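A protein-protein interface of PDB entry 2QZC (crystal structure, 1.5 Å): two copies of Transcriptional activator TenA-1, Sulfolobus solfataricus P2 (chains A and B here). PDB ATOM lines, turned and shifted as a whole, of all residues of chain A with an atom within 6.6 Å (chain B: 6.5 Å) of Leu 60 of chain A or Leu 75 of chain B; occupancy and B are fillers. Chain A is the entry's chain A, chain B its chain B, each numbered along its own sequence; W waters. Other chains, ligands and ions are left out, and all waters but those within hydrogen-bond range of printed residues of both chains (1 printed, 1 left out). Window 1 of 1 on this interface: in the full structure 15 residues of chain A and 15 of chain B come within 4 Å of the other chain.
The guanidinium group (NH1) of Arg 57 of chain A is in hydrogen-bond range of the backbone carbonyl oxygen (O) of Ser 64 of chain B (2.9 Å).
The side-chain amide nitrogen (ND2) of Asn 76 of chain B lies within hydrogen-bond range of the backbone carbonyl oxygen (O) of Phe 79 of chain A.
The backbone carbonyl oxygen (O) of Ser 64 of chain A lies within hydrogen-bond range of the guanidinium group (NH1) of Arg 57 of chain B, 3.0 Å away.
O of Ile 68 of chain B lies within hydrogen-bond range of OG1 of Thr 72 of chain B (2.7 Å).
OG of Ser 63 of chain B lies within hydrogen-bond range of O of Leu 59 of chain B, 3.1 Å away.
The backbone carbonyl oxygen (O) of Leu 60 of chain A sits at hydrogen-bond distance from the side-chain hydroxyl (OG) of Ser 63 of chain A (3.0 Å).
The side-chain hydroxyl (OG) of Ser 63 of chain A is in hydrogen-bond range of the backbone carbonyl oxygen (O) of Leu 59 of chain A, 3.0 Å away.
The side-chain hydroxyl (OG) of Ser 63 of chain B lies within hydrogen-bond range of the backbone carbonyl oxygen (O) of Leu 60 of chain B (2.9 Å).
The side-chain hydroxyl (OG) of Ser 64 of chain A sits at hydrogen-bond distance from the backbone carbonyl oxygen (O) of Ile 61 of chain A (2.6 Å).
Among the printed residues, pairs that only touch across the chains: Arg 57 of chain A with Lys 65 of chain B (3.9 Å), Arg 57 of chain A with Ile 68 of chain B (3.7 Å), Leu 60 of chain A with Leu 60 of chain B (3.5 Å), Leu 60 of chain A with Ser 63 of chain B (3.5 Å), Leu 60 of chain A with Leu 75 of chain B (3.7 Å), Ile 61 of chain A with Ser 64 of chain B (3.2 Å), Ser 63 of chain A with Leu 60 of chain B (3.6 Å), Ser 64 of chain A with Ile 61 of chain B (3.2 Å), Lys 65 of chain A with Arg 57 of chain B (3.9 Å), Leu 75 of chain A with Leu 60 of chain B (3.6 Å), Leu 75 of chain A with Phe 79 of chain B (3.9 Å) and Phe 79 of chain A with Leu 75 of chain B (3.6 Å).
Of the printed residues of chain B, Leu 60 of chain A touches Leu 60, Ser 63 and Leu 75.
Of the printed residues of chain B, Ser 64 of chain A touches Arg 57 and Ile 61.
Of the printed residues of chain A, Leu 60 of chain B touches Leu 60 (3.5 Å), Ser 63 (3.6 Å) and Leu 75 (3.6 Å).
Of the printed residues of chain A, Lys 65 of chain B touches Arg 57 (3.9 Å).
Of chain A, only Leu 60 and Phe 79 come within 4 Å of Leu 75 of chain B.
The nearest printed residue of chain B that does not touch Leu 60 of chain A is Ser 64 of chain B (4.1 Å).
Printed residues of chain A that touch a printed residue of chain B: Arg 57, Leu 60, Ile 61, Ser 63, Ser 64, Lys 65, Leu 75 and Phe 79.
Of the 19 printed residues of chain B, 10 touch a printed residue of chain A.
Printed residues of chain B that touch a printed residue of chain A: Arg 57, Leu 60, Ile 61, Ser 63, Ser 64, Lys 65, Ile 68, Leu 75, Asn 76 and Phe 79.
Hydrophobic or aromatic side chains of chain B that line the printed part of chain A: Leu 60, Ile 61, Ile 68, Leu 75 and Phe 79.
Along chain B the printed residues that touch a printed residue of chain A span positions 57 to 79.
Arg 57 of chain A touches Ser 64 of chain B, and with the chains exchanged Ser 64 of chain A touches Arg 57 of chain B.
Arg 57 of chain A touches Lys 65 of chain B, and with the chains exchanged Lys 65 of chain A touches Arg 57 of chain B.
Leu 60 of chain A touches Ser 63 of chain B, and with the chains exchanged Ser 63 of chain A touches Leu 60 of chain B.
Leu 75 of chain A touches Phe 79 of chain B, and with the chains exchanged Phe 79 of chain A touches Leu 75 of chain B.
Water W1 lies within hydrogen-bond range of N of Ile 68 of chain B (3.0 Å) and NH2 of Arg 57 of chain A (3.2 Å).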
ATOM      1  N   MET A  55      -8.501  35.851 -13.612  1.00  0.00           N
ATOM      2  CA  MET A  55      -7.015  35.947 -13.660  1.00  0.00           C
ATOM      3  C   MET A  55      -6.422  34.783 -14.470  1.00  0.00           C
ATOM      4  O   MET A  55      -5.530  34.983 -15.292  1.00  0.00           O
ATOM      5  CB  MET A  55      -6.465  35.926 -12.232  1.00  0.00           C
ATOM      6  CG  MET A  55      -5.021  36.144 -12.105  1.00  0.00           C
ATOM      7  SD  MET A  55      -4.325  35.410 -10.399  1.00  0.00           S
ATOM      8  CE  MET A  55      -4.320  33.540 -10.872  1.00  0.00           C
ATOM      9  N   LEU A  56      -6.939  33.585 -14.248  1.00  0.00           N
ATOM     10  CA  LEU A  56      -6.464  32.408 -14.988  1.00  0.00           C
ATOM     11  C   LEU A  56      -6.825  32.529 -16.457  1.00  0.00           C
ATOM     12  O   LEU A  56      -5.997  32.212 -17.353  1.00  0.00           O
ATOM     13  CB  LEU A  56      -7.042  31.125 -14.413  1.00  0.00           C
ATOM     14  CG  LEU A  56      -6.522  30.711 -13.050  1.00  0.00           C
ATOM     15  CD1 LEU A  56      -7.351  29.584 -12.480  1.00  0.00           C
ATOM     16  CD2 LEU A  56      -5.079  30.291 -13.126  1.00  0.00           C
ATOM     17  N   ARG A  57      -8.065  32.980 -16.758  1.00  0.00           N
ATOM     18  CA  ARG A  57      -8.427  33.167 -18.165  1.00  0.00           C
ATOM     19  C   ARG A  57      -7.531  34.184 -18.859  1.00  0.00           C
ATOM     20  O   ARG A  57      -7.072  33.996 -20.012  1.00  0.00           O
ATOM     21  CB  ARG A  57      -9.902  33.507 -18.296  1.00  0.00           C
ATOM     22  CG  ARG A  57     -10.810  32.346 -17.879  1.00  0.00           C
ATOM     23  CD  ARG A  57     -12.264  32.787 -18.004  1.00  0.00           C
ATOM     24  NE  ARG A  57     -13.220  31.768 -17.553  1.00  0.00           N
ATOM     25  CZ  ARG A  57     -13.625  30.723 -18.284  1.00  0.00           C
ATOM     26  NH1 ARG A  57     -13.177  30.541 -19.490  1.00  0.00           N
ATOM     27  NH2 ARG A  57     -14.514  29.860 -17.806  1.00  0.00           N
ATOM     28  N   ALA A  58      -7.257  35.287 -18.170  1.00  0.00           N
ATOM     29  CA  ALA A  58      -6.351  36.320 -18.701  1.00  0.00           C
ATOM     30  C   ALA A  58      -4.928  35.781 -18.900  1.00  0.00           C
ATOM     31  O   ALA A  58      -4.321  36.015 -19.944  1.00  0.00           O
ATOM     32  CB  ALA A  58      -6.373  37.535 -17.746  1.00  0.00           C
ATOM     33  N   LEU A  59      -4.448  34.999 -17.947  1.00  0.00           N
ATOM     34  CA  LEU A  59      -3.126  34.329 -18.090  1.00  0.00           C
ATOM     35  C   LEU A  59      -3.075  33.459 -19.345  1.00  0.00           C
ATOM     36  O   LEU A  59      -2.095  33.483 -20.092  1.00  0.00           O
ATOM     37  CB  LEU A  59      -2.794  33.454 -16.878  1.00  0.00           C
ATOM     38  CG  LEU A  59      -1.547  32.552 -16.928  1.00  0.00           C
ATOM     39  CD1 LEU A  59      -0.319  33.409 -17.182  1.00  0.00           C
ATOM     40  CD2 LEU A  59      -1.480  31.732 -15.651  1.00  0.00           C
ATOM     41  N   LEU A  60      -4.161  32.713 -19.570  1.00  0.00           N
ATOM     42  CA  LEU A  60      -4.187  31.826 -20.763  1.00  0.00           C
ATOM     43  C   LEU A  60      -4.087  32.628 -22.074  1.00  0.00           C
ATOM     44  O   LEU A  60      -3.229  32.324 -22.935  1.00  0.00           O
ATOM     45  CB  LEU A  60      -5.429  30.952 -20.748  1.00  0.00           C
ATOM     46  CG  LEU A  60      -5.457  29.877 -19.666  1.00  0.00           C
ATOM     47  CD1 LEU A  60      -6.896  29.306 -19.475  1.00  0.00           C
ATOM     48  CD2 LEU A  60      -4.423  28.767 -20.010  1.00  0.00           C
ATOM     49  N   ILE A  61      -4.865  33.714 -22.209  1.00  0.00           N
ATOM     50  CA  ILE A  61      -4.810  34.603 -23.387  1.00  0.00           C
ATOM     51  C   ILE A  61      -3.417  35.175 -23.526  1.00  0.00           C
ATOM     52  O   ILE A  61      -2.827  35.174 -24.618  1.00  0.00           O
ATOM     53  CB  ILE A  61      -5.791  35.867 -23.245  1.00  0.00           C
ATOM     54  CG1 ILE A  61      -7.246  35.471 -23.168  1.00  0.00           C
ATOM     55  CG2 ILE A  61      -5.583  36.845 -24.443  1.00  0.00           C
ATOM     56  CD1 ILE A  61      -8.169  36.579 -22.653  1.00  0.00           C
ATOM     57  N   ALA A  62      -2.886  35.710 -22.448  1.00  0.00           N
ATOM     58  CA  ALA A  62      -1.584  36.400 -22.493  1.00  0.00           C
ATOM     59  C   ALA A  62      -0.447  35.437 -22.822  1.00  0.00           C
ATOM     60  O   ALA A  62       0.453  35.779 -23.627  1.00  0.00           O
ATOM     61  CB  ALA A  62      -1.293  37.090 -21.158  1.00  0.00           C
ATOM     62  N   SER A  63      -0.497  34.261 -22.214  1.00  0.00           N
ATOM     63  CA  SER A  63       0.600  33.306 -22.366  1.00  0.00           C
ATOM     64  C   SER A  63       0.750  32.845 -23.821  1.00  0.00           C
ATOM     65  O   SER A  63       1.867  32.488 -24.234  1.00  0.00           O
ATOM     66  CB  SER A  63       0.456  32.136 -21.379  1.00  0.00           C
ATOM     67  OG  SER A  63      -0.674  31.358 -21.702  1.00  0.00           O
ATOM     68  N   SER A  64      -0.327  32.888 -24.596  1.00  0.00           N
ATOM     69  CA  SER A  64      -0.256  32.562 -26.032  1.00  0.00           C
ATOM     70  C   SER A  64       0.706  33.467 -26.795  1.00  0.00           C
ATOM     71  O   SER A  64       1.106  33.135 -27.934  1.00  0.00           O
ATOM     72  CB  SER A  64      -1.629  32.671 -26.683  1.00  0.00           C
ATOM     73  OG  SER A  64      -2.048  34.025 -26.851  1.00  0.00           O
ATOM     74  N   LYS A  65       1.060  34.627 -26.201  1.00  0.00           N
ATOM     75  CA  LYS A  65       1.913  35.640 -26.812  1.00  0.00           C
ATOM     76  C   LYS A  65       3.318  35.704 -26.235  1.00  0.00           C
ATOM     77  O   LYS A  65       4.110  36.519 -26.691  1.00  0.00           O
ATOM     78  CB  LYS A  65       1.273  37.035 -26.621  1.00  0.00           C
ATOM     79  CG  LYS A  65      -0.136  37.200 -27.185  1.00  0.00           C
ATOM     80  CD  LYS A  65      -0.715  38.574 -26.799  1.00  0.00           C
ATOM     81  CE  LYS A  65      -2.176  38.731 -27.235  1.00  0.00           C
ATOM     82  NZ  LYS A  65      -2.370  38.589 -28.699  1.00  0.00           N
ATOM     83  N   LEU A  75       2.991  27.749 -16.773  1.00  0.00           N
ATOM     84  CA  LEU A  75       1.757  26.954 -16.970  1.00  0.00           C
ATOM     85  C   LEU A  75       1.843  25.571 -16.328  1.00  0.00           C
ATOM     86  O   LEU A  75       0.847  25.090 -15.803  1.00  0.00           O
ATOM     87  CB  LEU A  75       1.369  26.865 -18.436  1.00  0.00           C
ATOM     88  CG  LEU A  75       0.985  28.189 -19.132  1.00  0.00           C
ATOM     89  CD1 LEU A  75       1.044  28.060 -20.642  1.00  0.00           C
ATOM     90  CD2 LEU A  75      -0.380  28.668 -18.670  1.00  0.00           C
ATOM     91  N   PHE A  79      -1.114  24.881 -13.659  1.00  0.00           N
ATOM     92  CA  PHE A  79      -2.016  23.755 -13.970  1.00  0.00           C
ATOM     93  C   PHE A  79      -1.531  22.379 -13.456  1.00  0.00           C
ATOM     94  O   PHE A  79      -1.902  21.351 -13.993  1.00  0.00           O
ATOM     95  CB  PHE A  79      -2.357  23.759 -15.469  1.00  0.00           C
ATOM     96  CG  PHE A  79      -3.181  24.916 -15.864  1.00  0.00           C
ATOM     97  CD1 PHE A  79      -4.552  24.917 -15.601  1.00  0.00           C
ATOM     98  CD2 PHE A  79      -2.613  26.042 -16.442  1.00  0.00           C
ATOM     99  CE1 PHE A  79      -5.332  26.005 -15.934  1.00  0.00           C
ATOM    100  CE2 PHE A  79      -3.376  27.139 -16.764  1.00  0.00           C
ATOM    101  CZ  PHE A  79      -4.754  27.120 -16.510  1.00  0.00           C
ATOM    102  N   ALA A 123      -3.943  41.421 -21.254  1.00  0.00           N
ATOM    103  CA  ALA A 123      -3.770  40.053 -21.833  1.00  0.00           C
ATOM    104  C   ALA A 123      -4.119  40.027 -23.293  1.00  0.00           C
ATOM    105  O   ALA A 123      -3.440  39.346 -24.093  1.00  0.00           O
ATOM    106  CB  ALA A 123      -4.609  39.066 -21.114  1.00  0.00           C
ATOM    107  N   PHE A 130       0.700  42.252 -19.720  1.00  0.00           N
ATOM    108  CA  PHE A 130      -0.040  41.403 -18.802  1.00  0.00           C
ATOM    109  C   PHE A 130       0.832  40.961 -17.634  1.00  0.00           C
ATOM    110  O   PHE A 130       0.418  40.992 -16.473  1.00  0.00           O
ATOM    111  CB  PHE A 130      -0.654  40.181 -19.486  1.00  0.00           C
ATOM    112  CG  PHE A 130      -1.205  39.178 -18.502  1.00  0.00           C
ATOM    113  CD1 PHE A 130      -2.418  39.421 -17.870  1.00  0.00           C
ATOM    114  CD2 PHE A 130      -0.428  38.074 -18.059  1.00  0.00           C
ATOM    115  CE1 PHE A 130      -2.895  38.544 -16.903  1.00  0.00           C
ATOM    116  CE2 PHE A 130      -0.909  37.232 -17.074  1.00  0.00           C
ATOM    117  CZ  PHE A 130      -2.129  37.475 -16.513  1.00  0.00           C
ATOM    118  N   ARG B  57      -0.164  27.478 -28.656  1.00  0.00           N
ATOM    119  CA  ARG B  57      -0.538  28.886 -28.463  1.00  0.00           C
ATOM    120  C   ARG B  57      -2.028  29.103 -28.766  1.00  0.00           C
ATOM    121  O   ARG B  57      -2.699  29.826 -28.033  1.00  0.00           O
ATOM    122  CB  ARG B  57       0.347  29.825 -29.304  1.00  0.00           C
ATOM    123  CG  ARG B  57       1.837  29.761 -28.933  1.00  0.00           C
ATOM    124  CD  ARG B  57       2.671  30.662 -29.869  1.00  0.00           C
ATOM    125  NE  ARG B  57       4.091  30.673 -29.484  1.00  0.00           N
ATOM    126  CZ  ARG B  57       4.638  31.414 -28.524  1.00  0.00           C
ATOM    127  NH1 ARG B  57       3.900  32.177 -27.765  1.00  0.00           N
ATOM    128  NH2 ARG B  57       5.933  31.334 -28.269  1.00  0.00           N
ATOM    129  N   LEU B  59      -4.394  26.790 -28.571  1.00  0.00           N
ATOM    130  CA  LEU B  59      -5.100  26.171 -27.431  1.00  0.00           C
ATOM    131  C   LEU B  59      -5.196  27.105 -26.248  1.00  0.00           C
ATOM    132  O   LEU B  59      -6.258  27.216 -25.615  1.00  0.00           O
ATOM    133  CB  LEU B  59      -4.409  24.877 -27.005  1.00  0.00           C
ATOM    134  CG  LEU B  59      -4.896  24.227 -25.712  1.00  0.00           C
ATOM    135  CD1 LEU B  59      -6.378  23.841 -25.795  1.00  0.00           C
ATOM    136  CD2 LEU B  59      -3.976  23.043 -25.349  1.00  0.00           C
ATOM    137  N   LEU B  60      -4.099  27.805 -25.940  1.00  0.00           N
ATOM    138  CA  LEU B  60      -4.076  28.743 -24.811  1.00  0.00           C
ATOM    139  C   LEU B  60      -5.110  29.848 -24.990  1.00  0.00           C
ATOM    140  O   LEU B  60      -5.937  30.095 -24.087  1.00  0.00           O
ATOM    141  CB  LEU B  60      -2.666  29.265 -24.533  1.00  0.00           C
ATOM    142  CG  LEU B  60      -1.668  28.215 -24.001  1.00  0.00           C
ATOM    143  CD1 LEU B  60      -0.225  28.697 -24.134  1.00  0.00           C
ATOM    144  CD2 LEU B  60      -1.986  27.850 -22.538  1.00  0.00           C
ATOM    145  N   ILE B  61      -5.112  30.477 -26.176  1.00  0.00           N
ATOM    146  CA  ILE B  61      -6.109  31.539 -26.475  1.00  0.00           C
ATOM    147  C   ILE B  61      -7.532  30.996 -26.395  1.00  0.00           C
ATOM    148  O   ILE B  61      -8.409  31.618 -25.802  1.00  0.00           O
ATOM    149  CB  ILE B  61      -5.987  32.060 -27.989  1.00  0.00           C
ATOM    150  CG1 ILE B  61      -4.632  32.677 -28.287  1.00  0.00           C
ATOM    151  CG2 ILE B  61      -7.072  33.135 -28.237  1.00  0.00           C
ATOM    152  CD1 ILE B  61      -4.287  32.797 -29.813  1.00  0.00           C
ATOM    153  N   SER B  63      -8.726  28.284 -24.870  1.00  0.00           N
ATOM    154  CA  SER B  63      -9.123  27.769 -23.561  1.00  0.00           C
ATOM    155  C   SER B  63      -9.606  28.896 -22.630  1.00  0.00           C
ATOM    156  O   SER B  63     -10.421  28.658 -21.721  1.00  0.00           O
ATOM    157  CB  SER B  63      -7.983  26.942 -22.945  1.00  0.00           C
ATOM    158  OG  SER B  63      -6.885  27.779 -22.638  1.00  0.00           O
ATOM    159  N   SER B  64      -9.134  30.123 -22.848  1.00  0.00           N
ATOM    160  CA  SER B  64      -9.595  31.235 -22.063  1.00  0.00           C
ATOM    161  C   SER B  64     -11.093  31.512 -22.187  1.00  0.00           C
ATOM    162  O   SER B  64     -11.656  32.195 -21.353  1.00  0.00           O
ATOM    163  CB  SER B  64      -8.885  32.545 -22.400  1.00  0.00           C
ATOM    164  OG  SER B  64      -9.313  33.037 -23.695  1.00  0.00           O
ATOM    165  N   LYS B  65     -11.703  30.968 -23.246  1.00  0.00           N
ATOM    166  CA  LYS B  65     -13.116  31.140 -23.545  1.00  0.00           C
ATOM    167  C   LYS B  65     -13.991  29.929 -23.231  1.00  0.00           C
ATOM    168  O   LYS B  65     -15.201  29.969 -23.494  1.00  0.00           O
ATOM    169  CB  LYS B  65     -13.249  31.437 -25.061  1.00  0.00           C
ATOM    170  CG  LYS B  65     -12.478  32.642 -25.534  1.00  0.00           C
ATOM    171  CD  LYS B  65     -12.411  32.656 -27.069  1.00  0.00           C
ATOM    172  CE  LYS B  65     -11.513  33.755 -27.566  1.00  0.00           C
ATOM    173  NZ  LYS B  65     -12.041  35.092 -27.170  1.00  0.00           N
ATOM    174  N   ILE B  68     -14.850  26.216 -17.500  1.00  0.00           N
ATOM    175  CA  ILE B  68     -13.674  26.151 -16.633  1.00  0.00           C
ATOM    176  C   ILE B  68     -13.246  24.719 -16.259  1.00  0.00           C
ATOM    177  O   ILE B  68     -12.041  24.403 -16.260  1.00  0.00           O
ATOM    178  CB  ILE B  68     -13.818  27.070 -15.377  1.00  0.00           C
ATOM    179  CG1 ILE B  68     -12.464  27.291 -14.690  1.00  0.00           C
ATOM    180  CG2 ILE B  68     -14.929  26.577 -14.395  1.00  0.00           C
ATOM    181  CD1 ILE B  68     -11.417  27.964 -15.580  1.00  0.00           C
ATOM    182  N   LYS B  70     -13.871  21.878 -17.973  1.00  0.00           N
ATOM    183  CA  LYS B  70     -13.399  21.144 -19.131  1.00  0.00           C
ATOM    184  C   LYS B  70     -12.016  21.589 -19.543  1.00  0.00           C
ATOM    185  O   LYS B  70     -11.151  20.753 -19.810  1.00  0.00           O
ATOM    186  CB  LYS B  70     -14.339  21.305 -20.328  1.00  0.00           C
ATOM    187  CG  LYS B  70     -15.763  20.801 -20.128  1.00  0.00           C
ATOM    188  CD  LYS B  70     -15.813  19.332 -19.840  1.00  0.00           C
ATOM    189  CE  LYS B  70     -17.227  18.828 -19.927  1.00  0.00           C
ATOM    190  NZ  LYS B  70     -18.160  19.521 -18.989  1.00  0.00           N
ATOM    191  N   VAL B  71     -11.797  22.910 -19.563  1.00  0.00           N
ATOM    192  CA  VAL B  71     -10.498  23.403 -20.019  1.00  0.00           C
ATOM    193  C   VAL B  71      -9.406  23.100 -18.996  1.00  0.00           C
ATOM    194  O   VAL B  71      -8.297  22.776 -19.405  1.00  0.00           O
ATOM    195  CB  VAL B  71     -10.526  24.897 -20.471  1.00  0.00           C
ATOM    196  CG1 VAL B  71     -11.580  25.069 -21.561  1.00  0.00           C
ATOM    197  CG2 VAL B  71     -10.754  25.862 -19.299  1.00  0.00           C
ATOM    198  N   THR B  72      -9.724  23.173 -17.700  1.00  0.00           N
ATOM    199  CA  THR B  72      -8.744  22.868 -16.649  1.00  0.00           C
ATOM    200  C   THR B  72      -8.253  21.412 -16.725  1.00  0.00           C
ATOM    201  O   THR B  72      -7.066  21.166 -16.570  1.00  0.00           O
ATOM    202  CB  THR B  72      -9.300  23.217 -15.254  1.00  0.00           C
ATOM    203  OG1 THR B  72      -9.564  24.635 -15.218  1.00  0.00           O
ATOM    204  CG2 THR B  72      -8.296  22.892 -14.186  1.00  0.00           C
ATOM    205  N   LYS B  73      -9.167  20.484 -17.005  1.00  0.00           N
ATOM    206  CA  LYS B  73      -8.834  19.062 -17.144  1.00  0.00           C
ATOM    207  C   LYS B  73      -7.875  18.849 -18.326  1.00  0.00           C
ATOM    208  O   LYS B  73      -6.877  18.132 -18.218  1.00  0.00           O
ATOM    209  CB  LYS B  73     -10.110  18.236 -17.326  1.00  0.00           C
ATOM    210  N   ILE B  74      -8.168  19.493 -19.455  1.00  0.00           N
ATOM    211  CA  ILE B  74      -7.319  19.405 -20.640  1.00  0.00           C
ATOM    212  C   ILE B  74      -5.943  20.017 -20.370  1.00  0.00           C
ATOM    213  O   ILE B  74      -4.921  19.374 -20.668  1.00  0.00           O
ATOM    214  CB  ILE B  74      -7.981  20.065 -21.908  1.00  0.00           C
ATOM    215  CG1 ILE B  74      -9.202  19.261 -22.348  1.00  0.00           C
ATOM    216  CG2 ILE B  74      -6.981  20.265 -23.076  1.00  0.00           C
ATOM    217  CD1 ILE B  74     -10.149  20.029 -23.267  1.00  0.00           C
ATOM    218  N   LEU B  75      -5.911  21.232 -19.818  1.00  0.00           N
ATOM    219  CA  LEU B  75      -4.632  21.928 -19.584  1.00  0.00           C
ATOM    220  C   LEU B  75      -3.735  21.193 -18.576  1.00  0.00           C
ATOM    221  O   LEU B  75      -2.515  21.194 -18.739  1.00  0.00           O
ATOM    222  CB  LEU B  75      -4.860  23.381 -19.167  1.00  0.00           C
ATOM    223  CG  LEU B  75      -5.544  24.296 -20.206  1.00  0.00           C
ATOM    224  CD1 LEU B  75      -6.088  25.534 -19.485  1.00  0.00           C
ATOM    225  CD2 LEU B  75      -4.626  24.666 -21.365  1.00  0.00           C
ATOM    226  N   ASN B  76      -4.342  20.579 -17.555  1.00  0.00           N
ATOM    227  CA  ASN B  76      -3.574  19.796 -16.580  1.00  0.00           C
ATOM    228  C   ASN B  76      -2.814  18.643 -17.253  1.00  0.00           C
ATOM    229  O   ASN B  76      -1.688  18.336 -16.854  1.00  0.00           O
ATOM    230  CB  ASN B  76      -4.466  19.267 -15.453  1.00  0.00           C
ATOM    231  CG  ASN B  76      -3.764  18.209 -14.598  1.00  0.00           C
ATOM    232  OD1 ASN B  76      -4.121  17.035 -14.653  1.00  0.00           O
ATOM    233  ND2 ASN B  76      -2.711  18.607 -13.896  1.00  0.00           N
ATOM    234  N   LEU B  77      -3.402  18.044 -18.284  1.00  0.00           N
ATOM    235  CA  LEU B  77      -2.768  16.933 -19.004  1.00  0.00           C
ATOM    236  C   LEU B  77      -1.785  17.399 -20.056  1.00  0.00           C
ATOM    237  O   LEU B  77      -0.759  16.763 -20.285  1.00  0.00           O
ATOM    238  CB  LEU B  77      -3.833  16.018 -19.618  1.00  0.00           C
ATOM    239  CG  LEU B  77      -4.770  15.371 -18.581  1.00  0.00           C
ATOM    240  CD1 LEU B  77      -5.873  14.612 -19.281  1.00  0.00           C
ATOM    241  CD2 LEU B  77      -4.034  14.473 -17.601  1.00  0.00           C
ATOM    242  N   VAL B  78      -2.098  18.508 -20.732  1.00  0.00           N
ATOM    243  CA  VAL B  78      -1.234  19.056 -21.765  1.00  0.00           C
ATOM    244  C   VAL B  78       0.036  19.664 -21.170  1.00  0.00           C
ATOM    245  O   VAL B  78       1.115  19.446 -21.693  1.00  0.00           O
ATOM    246  CB  VAL B  78      -1.985  20.091 -22.661  1.00  0.00           C
ATOM    247  CG1 VAL B  78      -0.987  20.861 -23.573  1.00  0.00           C
ATOM    248  CG2 VAL B  78      -3.035  19.381 -23.536  1.00  0.00           C
ATOM    249  N   PHE B  79      -0.097  20.442 -20.093  1.00  0.00           N
ATOM    250  CA  PHE B  79       1.068  21.052 -19.395  1.00  0.00           C
ATOM    251  C   PHE B  79       1.590  20.194 -18.210  1.00  0.00           C
ATOM    252  O   PHE B  79       2.151  20.720 -17.270  1.00  0.00           O
ATOM    253  CB  PHE B  79       0.771  22.532 -19.046  1.00  0.00           C
ATOM    254  CG  PHE B  79       0.589  23.371 -20.266  1.00  0.00           C
ATOM    255  CD1 PHE B  79       1.705  23.831 -20.975  1.00  0.00           C
ATOM    256  CD2 PHE B  79      -0.682  23.626 -20.777  1.00  0.00           C
ATOM    257  CE1 PHE B  79       1.557  24.551 -22.163  1.00  0.00           C
ATOM    258  CE2 PHE B  79      -0.852  24.342 -21.956  1.00  0.00           C
ATOM    259  CZ  PHE B  79       0.273  24.810 -22.664  1.00  0.00           C
ATOM    260  N   SER B  80       1.445  18.865 -18.303  1.00  0.00           N
ATOM    261  CA  SER B  80       1.939  17.908 -17.299  1.00  0.00           C
ATOM    262  C   SER B  80       3.434  17.619 -17.527  1.00  0.00           C
ATOM    263  O   SER B  80       4.034  18.076 -18.517  1.00  0.00           O
ATOM    264  CB  SER B  80       1.158  16.582 -17.400  1.00  0.00           C
ATOM    265  OG  SER B  80       1.607  15.615 -16.464  1.00  0.00           O
HETATM  266  O   HOH W   1     -17.080  28.115 -17.066  1.00  0.00           O
